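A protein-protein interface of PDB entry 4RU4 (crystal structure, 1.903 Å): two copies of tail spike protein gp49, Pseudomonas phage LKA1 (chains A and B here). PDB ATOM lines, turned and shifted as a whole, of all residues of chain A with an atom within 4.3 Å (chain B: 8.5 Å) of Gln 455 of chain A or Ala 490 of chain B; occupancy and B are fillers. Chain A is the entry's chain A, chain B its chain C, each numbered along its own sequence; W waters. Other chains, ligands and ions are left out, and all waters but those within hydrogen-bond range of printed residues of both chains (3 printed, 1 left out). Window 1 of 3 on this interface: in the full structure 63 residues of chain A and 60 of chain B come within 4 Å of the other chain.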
ATOM      1  N   PHE A 422     -15.276   2.164  -4.637  1.00  0.00           N
ATOM      2  CA  PHE A 422     -16.354   1.784  -3.752  1.00  0.00           C
ATOM      3  C   PHE A 422     -17.288   2.989  -3.636  1.00  0.00           C
ATOM      4  O   PHE A 422     -16.885   4.060  -3.173  1.00  0.00           O
ATOM      5  CB  PHE A 422     -15.786   1.342  -2.405  1.00  0.00           C
ATOM      6  CG  PHE A 422     -14.968   0.082  -2.505  1.00  0.00           C
ATOM      7  CD1 PHE A 422     -15.594  -1.163  -2.496  1.00  0.00           C
ATOM      8  CD2 PHE A 422     -13.577   0.132  -2.638  1.00  0.00           C
ATOM      9  CE1 PHE A 422     -14.841  -2.347  -2.608  1.00  0.00           C
ATOM     10  CE2 PHE A 422     -12.824  -1.047  -2.758  1.00  0.00           C
ATOM     11  CZ  PHE A 422     -13.455  -2.283  -2.747  1.00  0.00           C
ATOM     12  N   LEU A 423     -18.526   2.784  -4.063  1.00  0.00           N
ATOM     13  CA  LEU A 423     -19.511   3.849  -4.258  1.00  0.00           C
ATOM     14  C   LEU A 423     -20.726   3.614  -3.393  1.00  0.00           C
ATOM     15  O   LEU A 423     -21.414   2.596  -3.537  1.00  0.00           O
ATOM     16  CB  LEU A 423     -19.972   3.881  -5.738  1.00  0.00           C
ATOM     17  CG  LEU A 423     -18.880   3.920  -6.830  1.00  0.00           C
ATOM     18  CD1 LEU A 423     -19.530   4.041  -8.229  1.00  0.00           C
ATOM     19  CD2 LEU A 423     -17.815   5.023  -6.613  1.00  0.00           C
ATOM     20  N   ILE A 424     -20.996   4.551  -2.492  1.00  0.00           N
ATOM     21  CA  ILE A 424     -22.221   4.498  -1.708  1.00  0.00           C
ATOM     22  C   ILE A 424     -23.007   5.752  -2.113  1.00  0.00           C
ATOM     23  O   ILE A 424     -22.575   6.868  -1.833  1.00  0.00           O
ATOM     24  CB  ILE A 424     -21.950   4.472  -0.184  1.00  0.00           C
ATOM     25  CG1 ILE A 424     -21.264   3.161   0.254  1.00  0.00           C
ATOM     26  CG2 ILE A 424     -23.274   4.639   0.592  1.00  0.00           C
ATOM     27  CD1 ILE A 424     -19.815   3.047  -0.125  1.00  0.00           C
ATOM     28  N   GLN A 425     -24.123   5.572  -2.818  1.00  0.00           N
ATOM     29  CA  GLN A 425     -24.901   6.703  -3.316  1.00  0.00           C
ATOM     30  C   GLN A 425     -26.325   6.707  -2.782  1.00  0.00           C
ATOM     31  O   GLN A 425     -27.122   5.810  -3.102  1.00  0.00           O
ATOM     32  CB  GLN A 425     -24.934   6.713  -4.864  1.00  0.00           C
ATOM     33  CG  GLN A 425     -23.576   6.838  -5.517  1.00  0.00           C
ATOM     34  CD  GLN A 425     -23.637   6.841  -7.047  1.00  0.00           C
ATOM     35  OE1 GLN A 425     -24.696   6.627  -7.631  1.00  0.00           O
ATOM     36  NE2 GLN A 425     -22.503   7.078  -7.690  1.00  0.00           N
ATOM     37  N   ILE A 454     -12.951   5.994  -2.895  1.00  0.00           N
ATOM     38  CA  ILE A 454     -14.181   5.953  -2.114  1.00  0.00           C
ATOM     39  C   ILE A 454     -15.066   7.152  -2.471  1.00  0.00           C
ATOM     40  O   ILE A 454     -14.606   8.307  -2.427  1.00  0.00           O
ATOM     41  CB  ILE A 454     -13.901   6.069  -0.586  1.00  0.00           C
ATOM     42  CG1 ILE A 454     -12.807   5.096  -0.116  1.00  0.00           C
ATOM     43  CG2 ILE A 454     -15.191   5.802   0.198  1.00  0.00           C
ATOM     44  CD1 ILE A 454     -13.203   3.654  -0.215  1.00  0.00           C
ATOM     45  N   GLN A 455     -16.326   6.877  -2.807  1.00  0.00           N
ATOM     46  CA  GLN A 455     -17.340   7.918  -2.958  1.00  0.00           C
ATOM     47  C   GLN A 455     -18.471   7.606  -1.972  1.00  0.00           C
ATOM     48  O   GLN A 455     -19.217   6.634  -2.156  1.00  0.00           O
ATOM     49  CB  GLN A 455     -17.897   7.994  -4.393  1.00  0.00           C
ATOM     50  CG  GLN A 455     -19.075   9.004  -4.538  1.00  0.00           C
ATOM     51  CD  GLN A 455     -19.902   8.784  -5.810  1.00  0.00           C
ATOM     52  OE1 GLN A 455     -20.285   7.654  -6.147  1.00  0.00           O
ATOM     53  NE2 GLN A 455     -20.168   9.859  -6.522  1.00  0.00           N
ATOM     54  N   TYR A 456     -18.559   8.389  -0.905  1.00  0.00           N
ATOM     55  CA  TYR A 456     -19.585   8.156   0.112  1.00  0.00           C
ATOM     56  C   TYR A 456     -20.499   9.385   0.096  1.00  0.00           C
ATOM     57  O   TYR A 456     -20.150  10.415   0.634  1.00  0.00           O
ATOM     58  CB  TYR A 456     -18.945   7.924   1.491  1.00  0.00           C
ATOM     59  CG  TYR A 456     -19.822   7.135   2.427  1.00  0.00           C
ATOM     60  CD1 TYR A 456     -20.980   7.679   2.929  1.00  0.00           C
ATOM     61  CD2 TYR A 456     -19.500   5.827   2.794  1.00  0.00           C
ATOM     62  CE1 TYR A 456     -21.815   6.956   3.776  1.00  0.00           C
ATOM     63  CE2 TYR A 456     -20.332   5.095   3.638  1.00  0.00           C
ATOM     64  CZ  TYR A 456     -21.485   5.662   4.126  1.00  0.00           C
ATOM     65  OH  TYR A 456     -22.336   4.952   4.968  1.00  0.00           O
ATOM     66  N   SER A 457     -21.691   9.253  -0.497  1.00  0.00           N
ATOM     67  CA  SER A 457     -22.386  10.393  -1.098  1.00  0.00           C
ATOM     68  C   SER A 457     -23.928  10.320  -1.042  1.00  0.00           C
ATOM     69  O   SER A 457     -24.518   9.455  -1.676  1.00  0.00           O
ATOM     70  CB  SER A 457     -21.951  10.442  -2.561  1.00  0.00           C
ATOM     71  OG  SER A 457     -22.516  11.523  -3.258  1.00  0.00           O
ATOM     72  N   TYR A 483      -9.353   9.608  -5.861  1.00  0.00           N
ATOM     73  CA  TYR A 483     -10.288  10.417  -5.055  1.00  0.00           C
ATOM     74  C   TYR A 483     -10.740   9.752  -3.757  1.00  0.00           C
ATOM     75  O   TYR A 483     -10.819   8.531  -3.644  1.00  0.00           O
ATOM     76  CB  TYR A 483     -11.537  10.830  -5.868  1.00  0.00           C
ATOM     77  CG  TYR A 483     -12.384   9.681  -6.369  1.00  0.00           C
ATOM     78  CD1 TYR A 483     -13.367   9.100  -5.560  1.00  0.00           C
ATOM     79  CD2 TYR A 483     -12.235   9.201  -7.682  1.00  0.00           C
ATOM     80  CE1 TYR A 483     -14.165   8.051  -6.025  1.00  0.00           C
ATOM     81  CE2 TYR A 483     -13.032   8.148  -8.153  1.00  0.00           C
ATOM     82  CZ  TYR A 483     -13.985   7.575  -7.310  1.00  0.00           C
ATOM     83  OH  TYR A 483     -14.785   6.536  -7.760  1.00  0.00           O
ATOM     84  N   ILE A 485     -13.911  10.882  -1.226  1.00  0.00           N
ATOM     85  CA  ILE A 485     -15.011  11.844  -1.229  1.00  0.00           C
ATOM     86  C   ILE A 485     -16.058  11.487  -0.189  1.00  0.00           C
ATOM     87  O   ILE A 485     -16.579  10.378  -0.186  1.00  0.00           O
ATOM     88  CB  ILE A 485     -15.664  11.925  -2.633  1.00  0.00           C
ATOM     89  CG1 ILE A 485     -14.709  12.588  -3.632  1.00  0.00           C
ATOM     90  CG2 ILE A 485     -17.041  12.694  -2.587  1.00  0.00           C
ATOM     91  CD1 ILE A 485     -15.100  12.381  -5.144  1.00  0.00           C
ATOM     92  N   GLU A 487     -19.591  13.293   1.102  1.00  0.00           N
ATOM     93  CA  GLU A 487     -20.402  14.452   0.717  1.00  0.00           C
ATOM     94  C   GLU A 487     -21.877  14.215   0.958  1.00  0.00           C
ATOM     95  O   GLU A 487     -22.343  13.061   0.924  1.00  0.00           O
ATOM     96  CB  GLU A 487     -20.181  14.803  -0.755  1.00  0.00           C
ATOM     97  CG  GLU A 487     -20.740  13.770  -1.719  1.00  0.00           C
ATOM     98  CD  GLU A 487     -20.273  13.984  -3.168  1.00  0.00           C
ATOM     99  OE1 GLU A 487     -19.551  14.972  -3.438  1.00  0.00           O
ATOM    100  OE2 GLU A 487     -20.593  13.136  -4.032  1.00  0.00           O
ATOM    101  N   GLN B 386     -29.254   6.962 -12.088  1.00  0.00           N
ATOM    102  CA  GLN B 386     -28.416   5.945 -11.462  1.00  0.00           C
ATOM    103  C   GLN B 386     -28.082   4.787 -12.419  1.00  0.00           C
ATOM    104  O   GLN B 386     -28.234   3.624 -12.076  1.00  0.00           O
ATOM    105  CB  GLN B 386     -29.084   5.426 -10.176  1.00  0.00           C
ATOM    106  CG  GLN B 386     -29.589   6.538  -9.232  1.00  0.00           C
ATOM    107  CD  GLN B 386     -28.485   7.130  -8.381  1.00  0.00           C
ATOM    108  OE1 GLN B 386     -27.463   6.494  -8.169  1.00  0.00           O
ATOM    109  NE2 GLN B 386     -28.686   8.359  -7.892  1.00  0.00           N
ATOM    110  N   GLY B 426     -26.368  10.544 -10.469  1.00  0.00           N
ATOM    111  CA  GLY B 426     -25.671   9.418  -9.871  1.00  0.00           C
ATOM    112  C   GLY B 426     -25.177   8.360 -10.850  1.00  0.00           C
ATOM    113  O   GLY B 426     -24.920   8.646 -12.023  1.00  0.00           O
ATOM    114  N   GLY B 427     -25.004   7.140 -10.346  1.00  0.00           N
ATOM    115  CA  GLY B 427     -24.551   6.046 -11.190  1.00  0.00           C
ATOM    116  C   GLY B 427     -23.057   6.176 -11.480  1.00  0.00           C
ATOM    117  O   GLY B 427     -22.324   6.872 -10.766  1.00  0.00           O
ATOM    118  N   SER B 428     -22.614   5.531 -12.549  1.00  0.00           N
ATOM    119  CA  SER B 428     -21.217   5.592 -12.941  1.00  0.00           C
ATOM    120  C   SER B 428     -21.044   5.636 -14.446  1.00  0.00           C
ATOM    121  O   SER B 428     -21.922   5.224 -15.193  1.00  0.00           O
ATOM    122  CB  SER B 428     -20.420   4.413 -12.354  1.00  0.00           C
ATOM    123  OG  SER B 428     -20.952   3.184 -12.814  1.00  0.00           O
ATOM    124  N   LEU B 429     -19.889   6.126 -14.888  1.00  0.00           N
ATOM    125  CA  LEU B 429     -19.544   6.115 -16.306  1.00  0.00           C
ATOM    126  C   LEU B 429     -18.080   5.697 -16.406  1.00  0.00           C
ATOM    127  O   LEU B 429     -17.209   6.344 -15.821  1.00  0.00           O
ATOM    128  CB  LEU B 429     -19.747   7.521 -16.907  1.00  0.00           C
ATOM    129  CG  LEU B 429     -19.482   7.747 -18.406  1.00  0.00           C
ATOM    130  CD1 LEU B 429     -20.278   8.935 -18.898  1.00  0.00           C
ATOM    131  CD2 LEU B 429     -18.038   8.014 -18.686  1.00  0.00           C
ATOM    132  N   LEU B 440     -17.856  14.464 -22.137  1.00  0.00           N
ATOM    133  CA  LEU B 440     -18.833  13.503 -21.631  1.00  0.00           C
ATOM    134  C   LEU B 440     -20.232  13.751 -22.181  1.00  0.00           C
ATOM    135  O   LEU B 440     -20.950  12.810 -22.502  1.00  0.00           O
ATOM    136  CB  LEU B 440     -18.852  13.516 -20.098  1.00  0.00           C
ATOM    137  CG  LEU B 440     -17.543  13.047 -19.433  1.00  0.00           C
ATOM    138  CD1 LEU B 440     -17.719  13.036 -17.919  1.00  0.00           C
ATOM    139  CD2 LEU B 440     -17.143  11.663 -19.911  1.00  0.00           C
ATOM    140  N   TYR B 456     -25.873  17.773 -14.337  1.00  0.00           N
ATOM    141  CA  TYR B 456     -24.949  16.659 -14.440  1.00  0.00           C
ATOM    142  C   TYR B 456     -24.427  16.473 -13.015  1.00  0.00           C
ATOM    143  O   TYR B 456     -23.559  17.215 -12.571  1.00  0.00           O
ATOM    144  CB  TYR B 456     -23.810  16.987 -15.424  1.00  0.00           C
ATOM    145  CG  TYR B 456     -23.169  15.745 -15.986  1.00  0.00           C
ATOM    146  CD1 TYR B 456     -22.355  14.946 -15.193  1.00  0.00           C
ATOM    147  CD2 TYR B 456     -23.395  15.348 -17.302  1.00  0.00           C
ATOM    148  CE1 TYR B 456     -21.784  13.794 -15.681  1.00  0.00           C
ATOM    149  CE2 TYR B 456     -22.808  14.194 -17.811  1.00  0.00           C
ATOM    150  CZ  TYR B 456     -21.995  13.420 -16.995  1.00  0.00           C
ATOM    151  OH  TYR B 456     -21.404  12.258 -17.470  1.00  0.00           O
ATOM    152  N   SER B 457     -24.954  15.487 -12.307  1.00  0.00           N
ATOM    153  CA  SER B 457     -24.940  15.522 -10.837  1.00  0.00           C
ATOM    154  C   SER B 457     -24.709  14.164 -10.176  1.00  0.00           C
ATOM    155  O   SER B 457     -25.562  13.273 -10.285  1.00  0.00           O
ATOM    156  CB  SER B 457     -26.309  16.060 -10.400  1.00  0.00           C
ATOM    157  OG  SER B 457     -26.518  15.949  -9.007  1.00  0.00           O
ATOM    158  N   GLY B 458     -23.604  13.992  -9.446  1.00  0.00           N
ATOM    159  CA  GLY B 458     -23.486  12.813  -8.582  1.00  0.00           C
ATOM    160  C   GLY B 458     -22.790  11.583  -9.150  1.00  0.00           C
ATOM    161  O   GLY B 458     -22.553  10.592  -8.443  1.00  0.00           O
ATOM    162  N   GLN B 459     -22.453  11.630 -10.431  1.00  0.00           N
ATOM    163  CA  GLN B 459     -21.944  10.454 -11.132  1.00  0.00           C
ATOM    164  C   GLN B 459     -20.492  10.165 -10.753  1.00  0.00           C
ATOM    165  O   GLN B 459     -19.684  11.079 -10.597  1.00  0.00           O
ATOM    166  CB  GLN B 459     -22.037  10.701 -12.647  1.00  0.00           C
ATOM    167  CG  GLN B 459     -21.645   9.513 -13.575  1.00  0.00           C
ATOM    168  CD  GLN B 459     -21.673   9.952 -15.036  1.00  0.00           C
ATOM    169  OE1 GLN B 459     -20.827  10.731 -15.472  1.00  0.00           O
ATOM    170  NE2 GLN B 459     -22.670   9.493 -15.782  1.00  0.00           N
ATOM    171  N   ALA B 460     -20.160   8.886 -10.626  1.00  0.00           N
ATOM    172  CA  ALA B 460     -18.774   8.470 -10.456  1.00  0.00           C
ATOM    173  C   ALA B 460     -18.179   8.134 -11.833  1.00  0.00           C
ATOM    174  O   ALA B 460     -18.715   7.300 -12.564  1.00  0.00           O
ATOM    175  CB  ALA B 460     -18.695   7.262  -9.532  1.00  0.00           C
ATOM    176  N   ILE B 461     -17.072   8.778 -12.165  1.00  0.00           N
ATOM    177  CA  ILE B 461     -16.474   8.693 -13.510  1.00  0.00           C
ATOM    178  C   ILE B 461     -15.113   7.979 -13.462  1.00  0.00           C
ATOM    179  O   ILE B 461     -14.320   8.189 -12.537  1.00  0.00           O
ATOM    180  CB  ILE B 461     -16.327  10.134 -14.089  1.00  0.00           C
ATOM    181  CG1 ILE B 461     -17.710  10.701 -14.425  1.00  0.00           C
ATOM    182  CG2 ILE B 461     -15.445  10.186 -15.297  1.00  0.00           C
ATOM    183  CD1 ILE B 461     -17.788  12.224 -14.320  1.00  0.00           C
ATOM    184  N   ASP B 462     -14.854   7.127 -14.449  1.00  0.00           N
ATOM    185  CA  ASP B 462     -13.630   6.352 -14.496  1.00  0.00           C
ATOM    186  C   ASP B 462     -13.082   6.457 -15.911  1.00  0.00           C
ATOM    187  O   ASP B 462     -13.554   5.778 -16.815  1.00  0.00           O
ATOM    188  CB  ASP B 462     -13.937   4.900 -14.115  1.00  0.00           C
ATOM    189  CG  ASP B 462     -12.716   4.014 -14.089  1.00  0.00           C
ATOM    190  OD1 ASP B 462     -11.621   4.421 -14.540  1.00  0.00           O
ATOM    191  OD2 ASP B 462     -12.862   2.867 -13.621  1.00  0.00           O
ATOM    192  N   VAL B 463     -12.106   7.343 -16.092  1.00  0.00           N
ATOM    193  CA  VAL B 463     -11.540   7.629 -17.406  1.00  0.00           C
ATOM    194  C   VAL B 463     -10.010   7.587 -17.358  1.00  0.00           C
ATOM    195  O   VAL B 463      -9.416   7.627 -16.271  1.00  0.00           O
ATOM    196  CB  VAL B 463     -11.958   9.046 -17.911  1.00  0.00           C
ATOM    197  CG1 VAL B 463     -13.473   9.100 -18.210  1.00  0.00           C
ATOM    198  CG2 VAL B 463     -11.533  10.155 -16.929  1.00  0.00           C
ATOM    199  N   LEU B 466      -9.422  12.856 -20.684  1.00  0.00           N
ATOM    200  CA  LEU B 466     -10.712  13.492 -20.901  1.00  0.00           C
ATOM    201  C   LEU B 466     -10.460  14.946 -21.244  1.00  0.00           C
ATOM    202  O   LEU B 466      -9.512  15.542 -20.729  1.00  0.00           O
ATOM    203  CB  LEU B 466     -11.582  13.409 -19.631  1.00  0.00           C
ATOM    204  CG  LEU B 466     -12.982  14.026 -19.740  1.00  0.00           C
ATOM    205  CD1 LEU B 466     -13.817  13.322 -20.816  1.00  0.00           C
ATOM    206  CD2 LEU B 466     -13.721  13.920 -18.408  1.00  0.00           C
ATOM    207  N   GLU B 487     -22.182  19.045 -10.680  1.00  0.00           N
ATOM    208  CA  GLU B 487     -21.958  18.914  -9.234  1.00  0.00           C
ATOM    209  C   GLU B 487     -21.652  17.494  -8.801  1.00  0.00           C
ATOM    210  O   GLU B 487     -22.080  16.538  -9.441  1.00  0.00           O
ATOM    211  CB  GLU B 487     -23.173  19.426  -8.448  1.00  0.00           C
ATOM    212  CG  GLU B 487     -24.428  18.562  -8.642  1.00  0.00           C
ATOM    213  CD  GLU B 487     -25.703  19.246  -8.191  1.00  0.00           C
ATOM    214  OE1 GLU B 487     -25.625  20.381  -7.638  1.00  0.00           O
ATOM    215  OE2 GLU B 487     -26.785  18.662  -8.426  1.00  0.00           O
ATOM    216  N   ASN B 488     -20.907  17.374  -7.698  1.00  0.00           N
ATOM    217  CA  ASN B 488     -20.723  16.087  -7.011  1.00  0.00           C
ATOM    218  C   ASN B 488     -20.227  14.977  -7.925  1.00  0.00           C
ATOM    219  O   ASN B 488     -20.739  13.863  -7.882  1.00  0.00           O
ATOM    220  CB  ASN B 488     -22.035  15.659  -6.340  1.00  0.00           C
ATOM    221  CG  ASN B 488     -22.606  16.758  -5.431  1.00  0.00           C
ATOM    222  OD1 ASN B 488     -21.859  17.474  -4.777  1.00  0.00           O
ATOM    223  ND2 ASN B 488     -23.920  16.907  -5.426  1.00  0.00           N
ATOM    224  N   LEU B 489     -19.248  15.282  -8.761  1.00  0.00           N
ATOM    225  CA  LEU B 489     -18.741  14.278  -9.677  1.00  0.00           C
ATOM    226  C   LEU B 489     -17.494  13.666  -9.049  1.00  0.00           C
ATOM    227  O   LEU B 489     -16.653  14.396  -8.521  1.00  0.00           O
ATOM    228  CB  LEU B 489     -18.383  14.907 -11.011  1.00  0.00           C
ATOM    229  CG  LEU B 489     -19.549  15.521 -11.776  1.00  0.00           C
ATOM    230  CD1 LEU B 489     -19.084  15.963 -13.190  1.00  0.00           C
ATOM    231  CD2 LEU B 489     -20.723  14.541 -11.848  1.00  0.00           C
ATOM    232  N   ALA B 490     -17.394  12.339  -9.058  1.00  0.00           N
ATOM    233  CA  ALA B 490     -16.145  11.697  -8.646  1.00  0.00           C
ATOM    234  C   ALA B 490     -15.320  11.238  -9.855  1.00  0.00           C
ATOM    235  O   ALA B 490     -15.878  10.849 -10.866  1.00  0.00           O
ATOM    236  CB  ALA B 490     -16.447  10.506  -7.752  1.00  0.00           C
ATOM    237  N   GLY B 491     -13.995  11.278  -9.745  1.00  0.00           N
ATOM    238  CA  GLY B 491     -13.133  10.675 -10.752  1.00  0.00           C
ATOM    239  C   GLY B 491     -12.651  11.599 -11.879  1.00  0.00           C
ATOM    240  O   GLY B 491     -12.002  11.138 -12.811  1.00  0.00           O
ATOM    241  N   LEU B 492     -12.930  12.895 -11.796  1.00  0.00           N
ATOM    242  CA  LEU B 492     -12.430  13.807 -12.841  1.00  0.00           C
ATOM    243  C   LEU B 492     -10.917  13.993 -12.699  1.00  0.00           C
ATOM    244  O   LEU B 492     -10.423  14.253 -11.601  1.00  0.00           O
ATOM    245  CB  LEU B 492     -13.124  15.163 -12.779  1.00  0.00           C
ATOM    246  CG  LEU B 492     -14.645  15.187 -12.926  1.00  0.00           C
ATOM    247  CD1 LEU B 492     -15.169  16.565 -12.557  1.00  0.00           C
ATOM    248  CD2 LEU B 492     -15.041  14.812 -14.343  1.00  0.00           C
ATOM    249  N   PRO B 493     -10.173  13.829 -13.800  1.00  0.00           N
ATOM    250  CA  PRO B 493      -8.724  14.052 -13.771  1.00  0.00           C
ATOM    251  C   PRO B 493      -8.362  15.535 -13.845  1.00  0.00           C
ATOM    252  O   PRO B 493      -9.163  16.351 -14.305  1.00  0.00           O
ATOM    253  CB  PRO B 493      -8.231  13.330 -15.034  1.00  0.00           C
ATOM    254  CG  PRO B 493      -9.416  13.395 -15.977  1.00  0.00           C
ATOM    255  CD  PRO B 493     -10.641  13.292 -15.096  1.00  0.00           C
ATOM    256  N   ARG B 537      -7.479  22.878 -10.671  1.00  0.00           N
ATOM    257  CA  ARG B 537      -7.566  21.508 -11.158  1.00  0.00           C
ATOM    258  C   ARG B 537      -8.475  21.393 -12.386  1.00  0.00           C
ATOM    259  O   ARG B 537      -8.196  20.597 -13.293  1.00  0.00           O
ATOM    260  CB  ARG B 537      -8.096  20.607 -10.054  1.00  0.00           C
ATOM    261  CG  ARG B 537      -8.080  19.126 -10.404  1.00  0.00           C
ATOM    262  CD  ARG B 537      -8.728  18.274  -9.276  1.00  0.00           C
ATOM    263  NE  ARG B 537      -8.865  16.869  -9.685  1.00  0.00           N
ATOM    264  CZ  ARG B 537      -7.907  15.958  -9.574  1.00  0.00           C
ATOM    265  NH1 ARG B 537      -6.719  16.306  -9.073  1.00  0.00           N
ATOM    266  NH2 ARG B 537      -8.130  14.711  -9.967  1.00  0.00           N
ATOM    267  N   TYR B 538      -9.558  22.178 -12.418  1.00  0.00           N
ATOM    268  CA  TYR B 538     -10.508  22.171 -13.535  1.00  0.00           C
ATOM    269  C   TYR B 538     -10.631  23.587 -14.073  1.00  0.00           C
ATOM    270  O   TYR B 538     -10.545  24.543 -13.310  1.00  0.00           O
ATOM    271  CB  TYR B 538     -11.911  21.730 -13.105  1.00  0.00           C
ATOM    272  CG  TYR B 538     -11.938  20.446 -12.269  1.00  0.00           C
ATOM    273  CD1 TYR B 538     -11.147  19.357 -12.626  1.00  0.00           C
ATOM    274  CD2 TYR B 538     -12.770  20.326 -11.150  1.00  0.00           C
ATOM    275  CE1 TYR B 538     -11.153  18.185 -11.889  1.00  0.00           C
ATOM    276  CE2 TYR B 538     -12.785  19.130 -10.390  1.00  0.00           C
ATOM    277  CZ  TYR B 538     -11.965  18.079 -10.777  1.00  0.00           C
ATOM    278  OH  TYR B 538     -11.935  16.900 -10.072  1.00  0.00           O
HETATM  279  O   HOH W   1     -23.639  10.325  -5.757  1.00  0.00           O
HETATM  280  O   HOH W   2     -14.675   6.128 -10.495  1.00  0.00           O
HETATM  281  O   HOH W   3     -19.253  12.562  -6.048  1.00  0.00           O
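Ala 460 of chain B touches Leu 423 of chain A (CB to CD1, 3.6 Å). OE1 of Gln 425 of chain A touches C of Gly 426 of chain B (3.7 Å). Gln 425 of chain A touches Gly 458 of chain B. OE1 of Gln 455 of chain A touches CB of Ala 460 of chain B, 3.8 Å away. Gln 455 of chain A touches Ala 490 of chain B. CB of Ala 490 of chain B touches CE1 of Tyr 483 of chain A, 3.8 Å away. N of Gly 491 of chain B touches CD2 of Tyr 483 of chain A, at 3.4 Å. Ile 485 of chain A touches Ala 490 of chain B. OD1 of Asn 488 of chain B touches OE1 of Glu 487 of chain A (3.7 Å).
OE1 of Gln 386 of chain B lies close to OE1 of Gln 425 of chain A (2.8 Å). The side-chain amide oxygen of Gln 425 of chain A sits at hydrogen-bond distance from the backbone NH of Gly 427 of chain B, 2.8 Å away. The side-chain amide nitrogen (NE2) of Gln 455 of chain A sits at hydrogen-bond distance from the backbone carbonyl oxygen (O) of Gly 458 of chain B (3.1 Å).
Gln 455 of chain A touches just these residues of chain B: Gly 458 (3.1 Å), Ala 460 (3.8 Å) and Ala 490 (3.97 Å). Printed residues of chain B within 4 Å of Glu 487 of chain A: Asn 488. Printed residues of chain A within 4 Å of Gly 427 of chain B: Gln 425. Printed residues of chain A within 4 Å of Gly 458 of chain B: Gln 425 (3.6 Å) and Gln 455 (3.1 Å). Of the printed residues of chain A, Ala 460 of chain B touches Leu 423 (3.6 Å) and Gln 455 (3.8 Å). Ala 490 of chain B touches just these residues of chain A: Gln 455, Tyr 483 and Ile 485. The nearest printed residue of chain B that does not touch Gln 455 of chain A is Gln 459 of chain B (4.3 Å). The nearest printed residue of chain B that does not touch Glu 487 of chain A is Leu 489 of chain B (5.3 Å).
O of Gln 455 of chain A sits at hydrogen-bond distance from N of Ile 424 of chain A, 2.8 Å away. The side-chain amide oxygen (OE1) of Gln 455 of chain A is in hydrogen-bond range of the side-chain amide nitrogen (NE2) of Gln 425 of chain A, 2.8 Å away. O of Ile 454 of chain A sits at hydrogen-bond distance from N of Ile 485 of chain A (2.9 Å). The backbone NH (N) of Tyr 456 of chain A is in hydrogen-bond range of the backbone carbonyl oxygen (O) of Ile 485 of chain A (2.9 Å). The backbone carbonyl oxygen (O) of Gly 427 of chain B sits at hydrogen-bond distance from the backbone NH (N) of Ala 460 of chain B, at 3.0 Å. N of Leu 429 of chain B is in hydrogen-bond range of O of Ala 460 of chain B (2.9 Å).
Of the 24 printed residues of chain B, 8 touch a printed residue of chain A. Hydrophobic or aromatic side chains of chain B that line the printed part of chain A: Ala 460 and Ala 490. Of the 11 printed residues of chain A, 6 touch a printed residue of chain B. Hydrophobic or aromatic side chains of chain A that line the printed part of chain B: Leu 423, Tyr 483 and Ile 485. Along chain A the printed residues that touch a printed residue of chain B span positions 423 to 487. Among the printed residues, 12 pairs touch across the chains.
Positions printed for both chains: 456, 457 and 487. Of the 12 pairs that touch across the chains among the printed residues, none has its exchanged pair printed and touching as well.
Water W3 lies within hydrogen-bond range of the side-chain carboxylate (OE2) of Glu 487 of chain A (2.5 Å), the backbone carbonyl oxygen (O) of Asn 488 of chain B (2.7 Å) and the side-chain amide nitrogen (NE2) of Gln 455 of chain A (2.9 Å). Water W2 lies within hydrogen-bond range of OH of Tyr 483 of chain A (2.8 Å) and O of Ile 461 of chain B (2.9 Å). Water W1 lies within hydrogen-bond range of the backbone carbonyl oxygen (O) of Gly 458 of chain B and the side-chain hydroxyl (OG) of Ser 457 of chain A.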
